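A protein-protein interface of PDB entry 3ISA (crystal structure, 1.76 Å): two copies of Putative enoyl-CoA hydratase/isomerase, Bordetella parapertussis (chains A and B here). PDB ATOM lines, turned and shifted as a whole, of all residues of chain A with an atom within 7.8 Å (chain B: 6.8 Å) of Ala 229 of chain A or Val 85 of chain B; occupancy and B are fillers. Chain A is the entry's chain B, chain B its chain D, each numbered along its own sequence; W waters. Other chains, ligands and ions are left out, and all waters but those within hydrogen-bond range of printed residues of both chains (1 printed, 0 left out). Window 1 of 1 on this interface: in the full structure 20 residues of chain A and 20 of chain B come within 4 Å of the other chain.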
ATOM      1  N   GLU A  77      -2.445 -20.742  20.167  1.00  0.00           N
ATOM      2  CA  GLU A  77      -2.104 -21.321  18.871  1.00  0.00           C
ATOM      3  C   GLU A  77      -2.203 -20.256  17.777  1.00  0.00           C
ATOM      4  O   GLU A  77      -1.346 -20.183  16.895  1.00  0.00           O
ATOM      5  CB  GLU A  77      -3.036 -22.495  18.545  1.00  0.00           C
ATOM      6  CG  GLU A  77      -3.205 -23.522  19.683  1.00  0.00           C
ATOM      7  CD  GLU A  77      -2.314 -24.747  19.548  1.00  0.00           C
ATOM      8  OE1 GLU A  77      -2.640 -25.787  20.163  1.00  0.00           O
ATOM      9  OE2 GLU A  77      -1.297 -24.675  18.835  1.00  0.00           O
ATOM     10  N   GLY A  78      -3.237 -19.421  17.858  1.00  0.00           N
ATOM     11  CA  GLY A  78      -3.413 -18.307  16.916  1.00  0.00           C
ATOM     12  C   GLY A  78      -2.333 -17.239  16.990  1.00  0.00           C
ATOM     13  O   GLY A  78      -1.903 -16.723  15.962  1.00  0.00           O
ATOM     14  N   LEU A  80       0.723 -17.738  17.833  1.00  0.00           N
ATOM     15  CA  LEU A  80       1.927 -18.326  17.226  1.00  0.00           C
ATOM     16  C   LEU A  80       1.816 -18.379  15.701  1.00  0.00           C
ATOM     17  O   LEU A  80       2.784 -18.066  14.998  1.00  0.00           O
ATOM     18  CB  LEU A  80       2.195 -19.713  17.809  1.00  0.00           C
ATOM     19  CG  LEU A  80       2.475 -19.734  19.318  1.00  0.00           C
ATOM     20  CD1 LEU A  80       2.766 -21.154  19.785  1.00  0.00           C
ATOM     21  CD2 LEU A  80       3.619 -18.760  19.694  1.00  0.00           C
ATOM     22  N   LEU A  81       0.632 -18.737  15.197  1.00  0.00           N
ATOM     23  CA  LEU A  81       0.359 -18.677  13.753  1.00  0.00           C
ATOM     24  C   LEU A  81       0.617 -17.276  13.191  1.00  0.00           C
ATOM     25  O   LEU A  81       1.330 -17.143  12.197  1.00  0.00           O
ATOM     26  CB  LEU A  81      -1.081 -19.097  13.421  1.00  0.00           C
ATOM     27  CG  LEU A  81      -1.455 -18.876  11.946  1.00  0.00           C
ATOM     28  CD1 LEU A  81      -0.593 -19.721  10.955  1.00  0.00           C
ATOM     29  CD2 LEU A  81      -2.951 -19.068  11.703  1.00  0.00           C
ATOM     30  N   MET A  84       4.241 -16.402  12.929  1.00  0.00           N
ATOM     31  CA  MET A  84       4.844 -17.155  11.817  1.00  0.00           C
ATOM     32  C   MET A  84       4.450 -16.541  10.461  1.00  0.00           C
ATOM     33  O   MET A  84       5.290 -16.356   9.588  1.00  0.00           O
ATOM     34  CB  MET A  84       4.474 -18.648  11.909  1.00  0.00           C
ATOM     35  CG  MET A  84       5.345 -19.443  12.939  1.00  0.00           C
ATOM     36  SD  MET A  84       7.141 -19.473  12.627  1.00  0.00           S
ATOM     37  CE  MET A  84       7.621 -20.551  13.978  1.00  0.00           C
ATOM     38  N   VAL A  85       3.170 -16.193  10.295  1.00  0.00           N
ATOM     39  CA  VAL A  85       2.732 -15.494   9.076  1.00  0.00           C
ATOM     40  C   VAL A  85       3.487 -14.179   8.859  1.00  0.00           C
ATOM     41  O   VAL A  85       3.946 -13.900   7.742  1.00  0.00           O
ATOM     42  CB  VAL A  85       1.199 -15.296   9.078  1.00  0.00           C
ATOM     43  CG1 VAL A  85       0.742 -14.366   7.942  1.00  0.00           C
ATOM     44  CG2 VAL A  85       0.517 -16.671   8.993  1.00  0.00           C
ATOM     45  N   GLY A 139       6.616 -29.877  12.204  1.00  0.00           N
ATOM     46  CA  GLY A 139       5.651 -29.747  11.107  1.00  0.00           C
ATOM     47  C   GLY A 139       5.667 -28.407  10.380  1.00  0.00           C
ATOM     48  O   GLY A 139       4.858 -28.193   9.489  1.00  0.00           O
ATOM     49  N   LEU A 140       6.595 -27.520  10.739  1.00  0.00           N
ATOM     50  CA  LEU A 140       6.625 -26.161  10.182  1.00  0.00           C
ATOM     51  C   LEU A 140       7.228 -26.178   8.783  1.00  0.00           C
ATOM     52  O   LEU A 140       8.313 -26.722   8.593  1.00  0.00           O
ATOM     53  CB  LEU A 140       7.423 -25.224  11.094  1.00  0.00           C
ATOM     54  CG  LEU A 140       7.462 -23.776  10.600  1.00  0.00           C
ATOM     55  CD1 LEU A 140       6.051 -23.191  10.762  1.00  0.00           C
ATOM     56  CD2 LEU A 140       8.533 -22.922  11.288  1.00  0.00           C
ATOM     57  N   ALA A 222       0.932 -19.978   1.587  1.00  0.00           N
ATOM     58  CA  ALA A 222      -0.109 -21.006   1.793  1.00  0.00           C
ATOM     59  C   ALA A 222       0.447 -22.213   2.559  1.00  0.00           C
ATOM     60  O   ALA A 222      -0.152 -22.637   3.528  1.00  0.00           O
ATOM     61  CB  ALA A 222      -0.727 -21.456   0.475  1.00  0.00           C
ATOM     62  N   ALA A 223       1.614 -22.715   2.150  1.00  0.00           N
ATOM     63  CA  ALA A 223       2.229 -23.882   2.817  1.00  0.00           C
ATOM     64  C   ALA A 223       2.594 -23.542   4.257  1.00  0.00           C
ATOM     65  O   ALA A 223       2.396 -24.371   5.148  1.00  0.00           O
ATOM     66  CB  ALA A 223       3.469 -24.357   2.053  1.00  0.00           C
ATOM     67  N   LEU A 224       3.123 -22.335   4.483  1.00  0.00           N
ATOM     68  CA  LEU A 224       3.436 -21.880   5.846  1.00  0.00           C
ATOM     69  C   LEU A 224       2.194 -21.920   6.718  1.00  0.00           C
ATOM     70  O   LEU A 224       2.211 -22.519   7.801  1.00  0.00           O
ATOM     71  CB  LEU A 224       4.066 -20.467   5.864  1.00  0.00           C
ATOM     72  CG  LEU A 224       4.513 -19.858   7.222  1.00  0.00           C
ATOM     73  CD1 LEU A 224       3.362 -19.200   8.062  1.00  0.00           C
ATOM     74  CD2 LEU A 224       5.294 -20.873   8.101  1.00  0.00           C
ATOM     75  N   ALA A 225       1.135 -21.263   6.238  1.00  0.00           N
ATOM     76  CA  ALA A 225      -0.123 -21.112   6.974  1.00  0.00           C
ATOM     77  C   ALA A 225      -0.749 -22.464   7.324  1.00  0.00           C
ATOM     78  O   ALA A 225      -1.098 -22.691   8.486  1.00  0.00           O
ATOM     79  CB  ALA A 225      -1.090 -20.257   6.176  1.00  0.00           C
ATOM     80  N   ARG A 226      -0.843 -23.357   6.341  1.00  0.00           N
ATOM     81  CA  ARG A 226      -1.380 -24.709   6.560  1.00  0.00           C
ATOM     82  C   ARG A 226      -0.590 -25.449   7.640  1.00  0.00           C
ATOM     83  O   ARG A 226      -1.176 -26.044   8.534  1.00  0.00           O
ATOM     84  CB  ARG A 226      -1.411 -25.531   5.275  1.00  0.00           C
ATOM     85  CG  ARG A 226      -2.444 -25.040   4.283  1.00  0.00           C
ATOM     86  CD  ARG A 226      -2.759 -26.058   3.189  1.00  0.00           C
ATOM     87  NE  ARG A 226      -3.535 -25.405   2.131  1.00  0.00           N
ATOM     88  CZ  ARG A 226      -2.980 -24.899   1.029  1.00  0.00           C
ATOM     89  NH1 ARG A 226      -1.657 -25.003   0.852  1.00  0.00           N
ATOM     90  NH2 ARG A 226      -3.732 -24.316   0.103  1.00  0.00           N
ATOM     91  N   SER A 227       0.734 -25.359   7.556  1.00  0.00           N
ATOM     92  CA  SER A 227       1.635 -26.081   8.452  1.00  0.00           C
ATOM     93  C   SER A 227       1.505 -25.629   9.903  1.00  0.00           C
ATOM     94  O   SER A 227       1.442 -26.457  10.814  1.00  0.00           O
ATOM     95  CB  SER A 227       3.082 -25.951   7.954  1.00  0.00           C
ATOM     96  OG  SER A 227       3.675 -24.719   8.311  1.00  0.00           O
ATOM     97  N   ALA A 228       1.429 -24.319  10.105  1.00  0.00           N
ATOM     98  CA  ALA A 228       1.310 -23.728  11.449  1.00  0.00           C
ATOM     99  C   ALA A 228      -0.111 -23.723  11.999  1.00  0.00           C
ATOM    100  O   ALA A 228      -0.291 -23.590  13.222  1.00  0.00           O
ATOM    101  CB  ALA A 228       1.899 -22.312  11.461  1.00  0.00           C
ATOM    102  N   ALA A 229      -1.111 -23.851  11.124  1.00  0.00           N
ATOM    103  CA  ALA A 229      -2.513 -23.854  11.562  1.00  0.00           C
ATOM    104  C   ALA A 229      -3.095 -25.241  11.884  1.00  0.00           C
ATOM    105  O   ALA A 229      -4.246 -25.330  12.291  1.00  0.00           O
ATOM    106  CB  ALA A 229      -3.405 -23.155  10.535  1.00  0.00           C
ATOM    107  N   GLN A 230      -2.318 -26.306  11.683  1.00  0.00           N
ATOM    108  CA  GLN A 230      -2.787 -27.669  11.999  1.00  0.00           C
ATOM    109  C   GLN A 230      -2.968 -27.708  13.516  1.00  0.00           C
ATOM    110  O   GLN A 230      -2.063 -27.268  14.252  1.00  0.00           O
ATOM    111  CB  GLN A 230      -1.748 -28.732  11.599  1.00  0.00           C
ATOM    112  CG  GLN A 230      -1.363 -28.792  10.127  1.00  0.00           C
ATOM    113  CD  GLN A 230      -2.521 -29.173   9.197  1.00  0.00           C
ATOM    114  OE1 GLN A 230      -3.467 -29.858   9.599  1.00  0.00           O
ATOM    115  NE2 GLN A 230      -2.435 -28.741   7.938  1.00  0.00           N
ATOM    116  N   PRO A 231      -4.126 -28.196  13.999  1.00  0.00           N
ATOM    117  CA  PRO A 231      -4.321 -28.326  15.457  1.00  0.00           C
ATOM    118  C   PRO A 231      -3.169 -29.065  16.148  1.00  0.00           C
ATOM    119  O   PRO A 231      -2.567 -29.977  15.566  1.00  0.00           O
ATOM    120  CB  PRO A 231      -5.642 -29.095  15.571  1.00  0.00           C
ATOM    121  CG  PRO A 231      -6.394 -28.706  14.324  1.00  0.00           C
ATOM    122  CD  PRO A 231      -5.331 -28.609  13.243  1.00  0.00           C
ATOM    123  N   GLY A 232      -2.826 -28.619  17.351  1.00  0.00           N
ATOM    124  CA  GLY A 232      -1.734 -29.224  18.110  1.00  0.00           C
ATOM    125  C   GLY A 232      -0.365 -28.637  17.833  1.00  0.00           C
ATOM    126  O   GLY A 232       0.648 -29.258  18.174  1.00  0.00           O
ATOM    127  N   PHE A 233      -0.334 -27.448  17.222  1.00  0.00           N
ATOM    128  CA  PHE A 233       0.936 -26.735  16.916  1.00  0.00           C
ATOM    129  C   PHE A 233       1.856 -26.543  18.136  1.00  0.00           C
ATOM    130  O   PHE A 233       3.057 -26.903  18.088  1.00  0.00           O
ATOM    131  CB  PHE A 233       0.622 -25.384  16.231  1.00  0.00           C
ATOM    132  CG  PHE A 233       1.835 -24.665  15.672  1.00  0.00           C
ATOM    133  CD1 PHE A 233       2.815 -25.354  14.962  1.00  0.00           C
ATOM    134  CD2 PHE A 233       1.971 -23.287  15.831  1.00  0.00           C
ATOM    135  CE1 PHE A 233       3.934 -24.674  14.421  1.00  0.00           C
ATOM    136  CE2 PHE A 233       3.077 -22.607  15.306  1.00  0.00           C
ATOM    137  CZ  PHE A 233       4.053 -23.305  14.595  1.00  0.00           C
ATOM    138  N   ARG A 236       3.395 -29.807  19.257  1.00  0.00           N
ATOM    139  CA  ARG A 236       4.516 -30.215  18.396  1.00  0.00           C
ATOM    140  C   ARG A 236       5.801 -29.439  18.734  1.00  0.00           C
ATOM    141  O   ARG A 236       6.896 -30.018  18.767  1.00  0.00           O
ATOM    142  CB  ARG A 236       4.169 -30.032  16.919  1.00  0.00           C
ATOM    143  CG  ARG A 236       3.030 -30.895  16.431  1.00  0.00           C
ATOM    144  CD  ARG A 236       2.902 -30.821  14.915  1.00  0.00           C
ATOM    145  NE  ARG A 236       2.475 -29.515  14.394  1.00  0.00           N
ATOM    146  CZ  ARG A 236       1.205 -29.125  14.282  1.00  0.00           C
ATOM    147  NH1 ARG A 236       0.226 -29.927  14.681  1.00  0.00           N
ATOM    148  NH2 ARG A 236       0.913 -27.926  13.780  1.00  0.00           N
ATOM    149  N   VAL B  36     -16.540 -24.617  13.029  1.00  0.00           N
ATOM    150  CA  VAL B  36     -15.593 -24.802  11.908  1.00  0.00           C
ATOM    151  C   VAL B  36     -14.829 -26.111  12.092  1.00  0.00           C
ATOM    152  O   VAL B  36     -14.767 -26.927  11.159  1.00  0.00           O
ATOM    153  CB  VAL B  36     -14.656 -23.584  11.747  1.00  0.00           C
ATOM    154  CG1 VAL B  36     -13.527 -23.818  10.675  1.00  0.00           C
ATOM    155  CG2 VAL B  36     -15.483 -22.352  11.408  1.00  0.00           C
ATOM    156  N   GLU B  37     -14.299 -26.348  13.295  1.00  0.00           N
ATOM    157  CA  GLU B  37     -13.563 -27.599  13.543  1.00  0.00           C
ATOM    158  C   GLU B  37     -14.421 -28.868  13.377  1.00  0.00           C
ATOM    159  O   GLU B  37     -13.944 -29.874  12.864  1.00  0.00           O
ATOM    160  CB  GLU B  37     -12.851 -27.594  14.898  1.00  0.00           C
ATOM    161  CG  GLU B  37     -11.706 -26.586  15.026  1.00  0.00           C
ATOM    162  CD  GLU B  37     -10.663 -26.647  13.903  1.00  0.00           C
ATOM    163  OE1 GLU B  37     -10.163 -27.743  13.569  1.00  0.00           O
ATOM    164  OE2 GLU B  37     -10.326 -25.564  13.374  1.00  0.00           O
ATOM    165  N   ILE B  40     -14.820 -29.375   9.603  1.00  0.00           N
ATOM    166  CA  ILE B  40     -13.592 -29.923   9.061  1.00  0.00           C
ATOM    167  C   ILE B  40     -13.473 -31.429   9.360  1.00  0.00           C
ATOM    168  O   ILE B  40     -13.171 -32.206   8.451  1.00  0.00           O
ATOM    169  CB  ILE B  40     -12.355 -29.133   9.586  1.00  0.00           C
ATOM    170  CG1 ILE B  40     -12.281 -27.758   8.886  1.00  0.00           C
ATOM    171  CG2 ILE B  40     -11.085 -29.892   9.314  1.00  0.00           C
ATOM    172  CD1 ILE B  40     -11.277 -26.780   9.464  1.00  0.00           C
ATOM    173  N   LEU B  80      -8.002 -14.577  15.906  1.00  0.00           N
ATOM    174  CA  LEU B  80      -8.924 -14.259  14.811  1.00  0.00           C
ATOM    175  C   LEU B  80      -8.364 -14.725  13.465  1.00  0.00           C
ATOM    176  O   LEU B  80      -9.105 -15.268  12.630  1.00  0.00           O
ATOM    177  CB  LEU B  80      -9.223 -12.758  14.775  1.00  0.00           C
ATOM    178  CG  LEU B  80      -9.898 -12.220  16.044  1.00  0.00           C
ATOM    179  CD1 LEU B  80     -10.002 -10.700  15.952  1.00  0.00           C
ATOM    180  CD2 LEU B  80     -11.261 -12.872  16.302  1.00  0.00           C
ATOM    181  N   LEU B  81      -7.065 -14.516  13.271  1.00  0.00           N
ATOM    182  CA  LEU B  81      -6.363 -15.011  12.077  1.00  0.00           C
ATOM    183  C   LEU B  81      -6.487 -16.529  11.938  1.00  0.00           C
ATOM    184  O   LEU B  81      -6.838 -17.017  10.868  1.00  0.00           O
ATOM    185  CB  LEU B  81      -4.880 -14.604  12.072  1.00  0.00           C
ATOM    186  CG  LEU B  81      -4.064 -15.252  10.931  1.00  0.00           C
ATOM    187  CD1 LEU B  81      -4.530 -14.794   9.526  1.00  0.00           C
ATOM    188  CD2 LEU B  81      -2.548 -15.075  11.087  1.00  0.00           C
ATOM    189  N   LEU B  82      -6.208 -17.261  13.017  1.00  0.00           N
ATOM    190  CA  LEU B  82      -6.328 -18.718  13.015  1.00  0.00           C
ATOM    191  C   LEU B  82      -7.742 -19.161  12.612  1.00  0.00           C
ATOM    192  O   LEU B  82      -7.904 -20.037  11.762  1.00  0.00           O
ATOM    193  CB  LEU B  82      -5.905 -19.326  14.354  1.00  0.00           C
ATOM    194  CG  LEU B  82      -6.032 -20.858  14.453  1.00  0.00           C
ATOM    195  CD1 LEU B  82      -5.286 -21.545  13.312  1.00  0.00           C
ATOM    196  CD2 LEU B  82      -5.500 -21.372  15.796  1.00  0.00           C
ATOM    197  N   ARG B  83      -8.752 -18.526  13.196  1.00  0.00           N
ATOM    198  CA  ARG B  83     -10.125 -18.876  12.875  1.00  0.00           C
ATOM    199  C   ARG B  83     -10.475 -18.631  11.384  1.00  0.00           C
ATOM    200  O   ARG B  83     -11.165 -19.439  10.755  1.00  0.00           O
ATOM    201  CB  ARG B  83     -11.107 -18.172  13.825  1.00  0.00           C
ATOM    202  CG  ARG B  83     -11.096 -18.731  15.258  1.00  0.00           C
ATOM    203  CD  ARG B  83     -11.972 -17.879  16.178  1.00  0.00           C
ATOM    204  NE  ARG B  83     -13.356 -17.832  15.691  1.00  0.00           N
ATOM    205  CZ  ARG B  83     -14.266 -16.954  16.096  1.00  0.00           C
ATOM    206  NH1 ARG B  83     -13.939 -16.029  16.990  1.00  0.00           N
ATOM    207  NH2 ARG B  83     -15.498 -16.987  15.588  1.00  0.00           N
ATOM    208  N   MET B  84      -9.985 -17.532  10.825  1.00  0.00           N
ATOM    209  CA  MET B  84     -10.168 -17.259   9.396  1.00  0.00           C
ATOM    210  C   MET B  84      -9.411 -18.250   8.494  1.00  0.00           C
ATOM    211  O   MET B  84      -9.938 -18.709   7.486  1.00  0.00           O
ATOM    212  CB  MET B  84      -9.782 -15.807   9.088  1.00  0.00           C
ATOM    213  CG  MET B  84     -10.842 -14.778   9.515  1.00  0.00           C
ATOM    214  SD  MET B  84     -12.483 -14.954   8.768  1.00  0.00           S
ATOM    215  CE  MET B  84     -13.144 -13.399   9.396  1.00  0.00           C
ATOM    216  N   VAL B  85      -8.176 -18.591   8.876  1.00  0.00           N
ATOM    217  CA  VAL B  85      -7.395 -19.593   8.161  1.00  0.00           C
ATOM    218  C   VAL B  85      -8.081 -20.951   8.157  1.00  0.00           C
ATOM    219  O   VAL B  85      -8.192 -21.577   7.102  1.00  0.00           O
ATOM    220  CB  VAL B  85      -5.930 -19.666   8.713  1.00  0.00           C
ATOM    221  CG1 VAL B  85      -5.222 -20.909   8.194  1.00  0.00           C
ATOM    222  CG2 VAL B  85      -5.180 -18.385   8.300  1.00  0.00           C
ATOM    223  N   ARG B  86      -8.594 -21.367   9.321  1.00  0.00           N
ATOM    224  CA  ARG B  86      -9.315 -22.631   9.419  1.00  0.00           C
ATOM    225  C   ARG B  86     -10.607 -22.617   8.577  1.00  0.00           C
ATOM    226  O   ARG B  86     -10.946 -23.617   7.956  1.00  0.00           O
ATOM    227  CB  ARG B  86      -9.553 -23.022  10.890  1.00  0.00           C
ATOM    228  CG  ARG B  86      -8.248 -23.286  11.716  1.00  0.00           C
ATOM    229  CD  ARG B  86      -7.423 -24.462  11.180  1.00  0.00           C
ATOM    230  NE  ARG B  86      -8.035 -25.745  11.549  1.00  0.00           N
ATOM    231  CZ  ARG B  86      -7.700 -26.923  11.023  1.00  0.00           C
ATOM    232  NH1 ARG B  86      -6.763 -26.986  10.081  1.00  0.00           N
ATOM    233  NH2 ARG B  86      -8.298 -28.038  11.438  1.00  0.00           N
ATOM    234  N   ILE B  87     -11.313 -21.486   8.557  1.00  0.00           N
ATOM    235  CA  ILE B  87     -12.456 -21.312   7.649  1.00  0.00           C
ATOM    236  C   ILE B  87     -12.019 -21.520   6.190  1.00  0.00           C
ATOM    237  O   ILE B  87     -12.619 -22.317   5.474  1.00  0.00           O
ATOM    238  CB  ILE B  87     -13.178 -19.945   7.867  1.00  0.00           C
ATOM    239  CG1 ILE B  87     -13.971 -19.979   9.184  1.00  0.00           C
ATOM    240  CG2 ILE B  87     -14.135 -19.636   6.710  1.00  0.00           C
ATOM    241  CD1 ILE B  87     -14.446 -18.606   9.686  1.00  0.00           C
ATOM    242  N   GLU B  88     -10.954 -20.847   5.752  1.00  0.00           N
ATOM    243  CA  GLU B  88     -10.497 -21.034   4.357  1.00  0.00           C
ATOM    244  C   GLU B  88     -10.052 -22.476   4.079  1.00  0.00           C
ATOM    245  O   GLU B  88     -10.308 -22.998   2.998  1.00  0.00           O
ATOM    246  CB  GLU B  88      -9.398 -20.029   3.980  1.00  0.00           C
ATOM    247  CG  GLU B  88      -8.840 -20.131   2.522  1.00  0.00           C
ATOM    248  CD  GLU B  88      -9.898 -19.928   1.406  1.00  0.00           C
ATOM    249  OE1 GLU B  88     -11.067 -19.588   1.688  1.00  0.00           O
ATOM    250  OE2 GLU B  88      -9.550 -20.120   0.222  1.00  0.00           O
ATOM    251  N   MET B  89      -9.412 -23.123   5.060  1.00  0.00           N
ATOM    252  CA  MET B  89      -9.022 -24.512   4.905  1.00  0.00           C
ATOM    253  C   MET B  89     -10.279 -25.405   4.722  1.00  0.00           C
ATOM    254  O   MET B  89     -10.315 -26.275   3.846  1.00  0.00           O
ATOM    255  CB  MET B  89      -8.096 -24.964   6.044  1.00  0.00           C
ATOM    256  CG  MET B  89      -6.664 -24.330   5.966  1.00  0.00           C
ATOM    257  SD  MET B  89      -5.561 -24.699   7.376  1.00  0.00           S
ATOM    258  CE  MET B  89      -5.081 -26.355   6.957  1.00  0.00           C
ATOM    259  N   LEU B  90     -11.318 -25.127   5.504  1.00  0.00           N
ATOM    260  CA  LEU B  90     -12.601 -25.798   5.363  1.00  0.00           C
ATOM    261  C   LEU B  90     -13.214 -25.576   3.972  1.00  0.00           C
ATOM    262  O   LEU B  90     -13.637 -26.545   3.318  1.00  0.00           O
ATOM    263  CB  LEU B  90     -13.584 -25.333   6.445  1.00  0.00           C
ATOM    264  CG  LEU B  90     -15.031 -25.831   6.257  1.00  0.00           C
ATOM    265  CD1 LEU B  90     -15.159 -27.379   6.326  1.00  0.00           C
ATOM    266  CD2 LEU B  90     -15.996 -25.127   7.225  1.00  0.00           C
ATOM    267  N   LEU B  91     -13.237 -24.324   3.520  1.00  0.00           N
ATOM    268  CA  LEU B  91     -13.839 -23.985   2.219  1.00  0.00           C
ATOM    269  C   LEU B  91     -13.124 -24.718   1.070  1.00  0.00           C
ATOM    270  O   LEU B  91     -13.751 -25.218   0.137  1.00  0.00           O
ATOM    271  CB  LEU B  91     -13.825 -22.460   2.017  1.00  0.00           C
ATOM    272  CG  LEU B  91     -14.610 -21.661   3.058  1.00  0.00           C
ATOM    273  CD1 LEU B  91     -14.414 -20.163   2.850  1.00  0.00           C
ATOM    274  CD2 LEU B  91     -16.087 -22.053   3.010  1.00  0.00           C
ATOM    275  N   LEU B 221      -5.504 -19.052  -0.204  1.00  0.00           N
ATOM    276  CA  LEU B 221      -5.067 -19.080   1.179  1.00  0.00           C
ATOM    277  C   LEU B 221      -4.053 -17.962   1.472  1.00  0.00           C
ATOM    278  O   LEU B 221      -4.147 -17.312   2.522  1.00  0.00           O
ATOM    279  CB  LEU B 221      -4.537 -20.466   1.588  1.00  0.00           C
ATOM    280  CG  LEU B 221      -4.238 -20.554   3.095  1.00  0.00           C
ATOM    281  CD1 LEU B 221      -5.455 -20.236   3.988  1.00  0.00           C
ATOM    282  CD2 LEU B 221      -3.677 -21.911   3.456  1.00  0.00           C
ATOM    283  N   LEU B 224      -6.019 -14.662   1.715  1.00  0.00           N
ATOM    284  CA  LEU B 224      -6.722 -14.647   3.011  1.00  0.00           C
ATOM    285  C   LEU B 224      -5.764 -14.307   4.163  1.00  0.00           C
ATOM    286  O   LEU B 224      -6.034 -13.401   4.970  1.00  0.00           O
ATOM    287  CB  LEU B 224      -7.459 -15.978   3.273  1.00  0.00           C
ATOM    288  CG  LEU B 224      -8.298 -16.168   4.561  1.00  0.00           C
ATOM    289  CD1 LEU B 224      -7.446 -16.576   5.803  1.00  0.00           C
ATOM    290  CD2 LEU B 224      -9.129 -14.914   4.882  1.00  0.00           C
ATOM    291  N   ALA B 225      -4.661 -15.057   4.238  1.00  0.00           N
ATOM    292  CA  ALA B 225      -3.682 -14.927   5.303  1.00  0.00           C
ATOM    293  C   ALA B 225      -3.152 -13.500   5.387  1.00  0.00           C
ATOM    294  O   ALA B 225      -3.182 -12.912   6.465  1.00  0.00           O
ATOM    295  CB  ALA B 225      -2.515 -15.949   5.112  1.00  0.00           C
ATOM    296  N   ALA B 228      -5.962 -10.906   6.676  1.00  0.00           N
ATOM    297  CA  ALA B 228      -6.305 -11.013   8.093  1.00  0.00           C
ATOM    298  C   ALA B 228      -5.094 -10.774   9.030  1.00  0.00           C
ATOM    299  O   ALA B 228      -5.270 -10.529  10.220  1.00  0.00           O
ATOM    300  CB  ALA B 228      -6.950 -12.358   8.367  1.00  0.00           C
HETATM  301  O   HOH W   1      -5.997 -29.619   9.024  1.00  0.00           O
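N of Phe 233 of chain A lies close to OE2 of Glu 77 of chain A, at 3.3 Å. The side-chain amide nitrogen (NE2) of Gln 230 of chain A lies within hydrogen-bond range of the backbone carbonyl oxygen (O) of Arg 226 of chain A (3.0 Å). The guanidinium group of Arg 236 of chain A is in hydrogen-bond range of the backbone carbonyl oxygen of Gln 230 of chain A (3.1 Å). The backbone carbonyl oxygen (O) of Pro 231 of chain A sits at hydrogen-bond distance from the guanidinium group (NH1) of Arg 236 of chain A, 2.9 Å away. NH2 of Arg 86 of chain B is in salt-bridge range of OE1 of Glu 37 of chain B, at 2.8 Å. NH1 of Arg 86 of chain B lies close to SD of Met 89 of chain B, 3.7 Å away.
N of Gly 78 of chain A touches CD2 of Leu 82 of chain B, at 3.6 Å. Leu 82 of chain B touches Leu 81 of chain A. Leu 221 of chain B touches Ala 222 of chain A. Met 89 of chain B touches Arg 226 of chain A. Leu 221 of chain B touches Arg 226 of chain A. CD1 of Leu 82 of chain B touches CB of Ala 229 of chain A, 3.7 Å away. O of Ala 229 of chain A touches CD of Arg 86 of chain B, 3.5 Å away. Met 89 of chain B touches Gln 230 of chain A. Glu 37 of chain B touches Pro 231 of chain A. CD of Pro 231 of chain A touches NH2 of Arg 86 of chain B, at 3.5 Å.
Printed residues of chain B within 4 Å of Gln 230 of chain A: Met 89. Of the printed residues of chain A, Glu 37 of chain B touches Pro 231. Of chain A, only Ala 229 (3.7 Å) comes within 4 Å of Val 85 of chain B. The nearest residue of chain A that does not touch Val 85 of chain B is Leu 81 of chain A (4.1 Å). The nearest printed residue of chain A that does not touch Leu 82 of chain B is Ala 228 of chain A (5.4 Å).
Hydrophobic or aromatic side chains of chain A within 4 Å of the printed part of chain B: Leu 81, Ala 229 and Pro 231. Of the 19 printed residues of chain B, 6 touch a printed residue of chain A. Printed residues of chain B that touch a printed residue of chain A: Glu 37, Leu 82, Val 85, Arg 86, Met 89 and Leu 221. Hydrophobic or aromatic side chains of chain B that line the printed part of chain A: Leu 82, Val 85, Met 89 and Leu 221.
7 positions are printed for both chains.
Water W1 lies within hydrogen-bond range of OE1 of Gln 230 of chain A and NH1 of Arg 86 of chain B.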
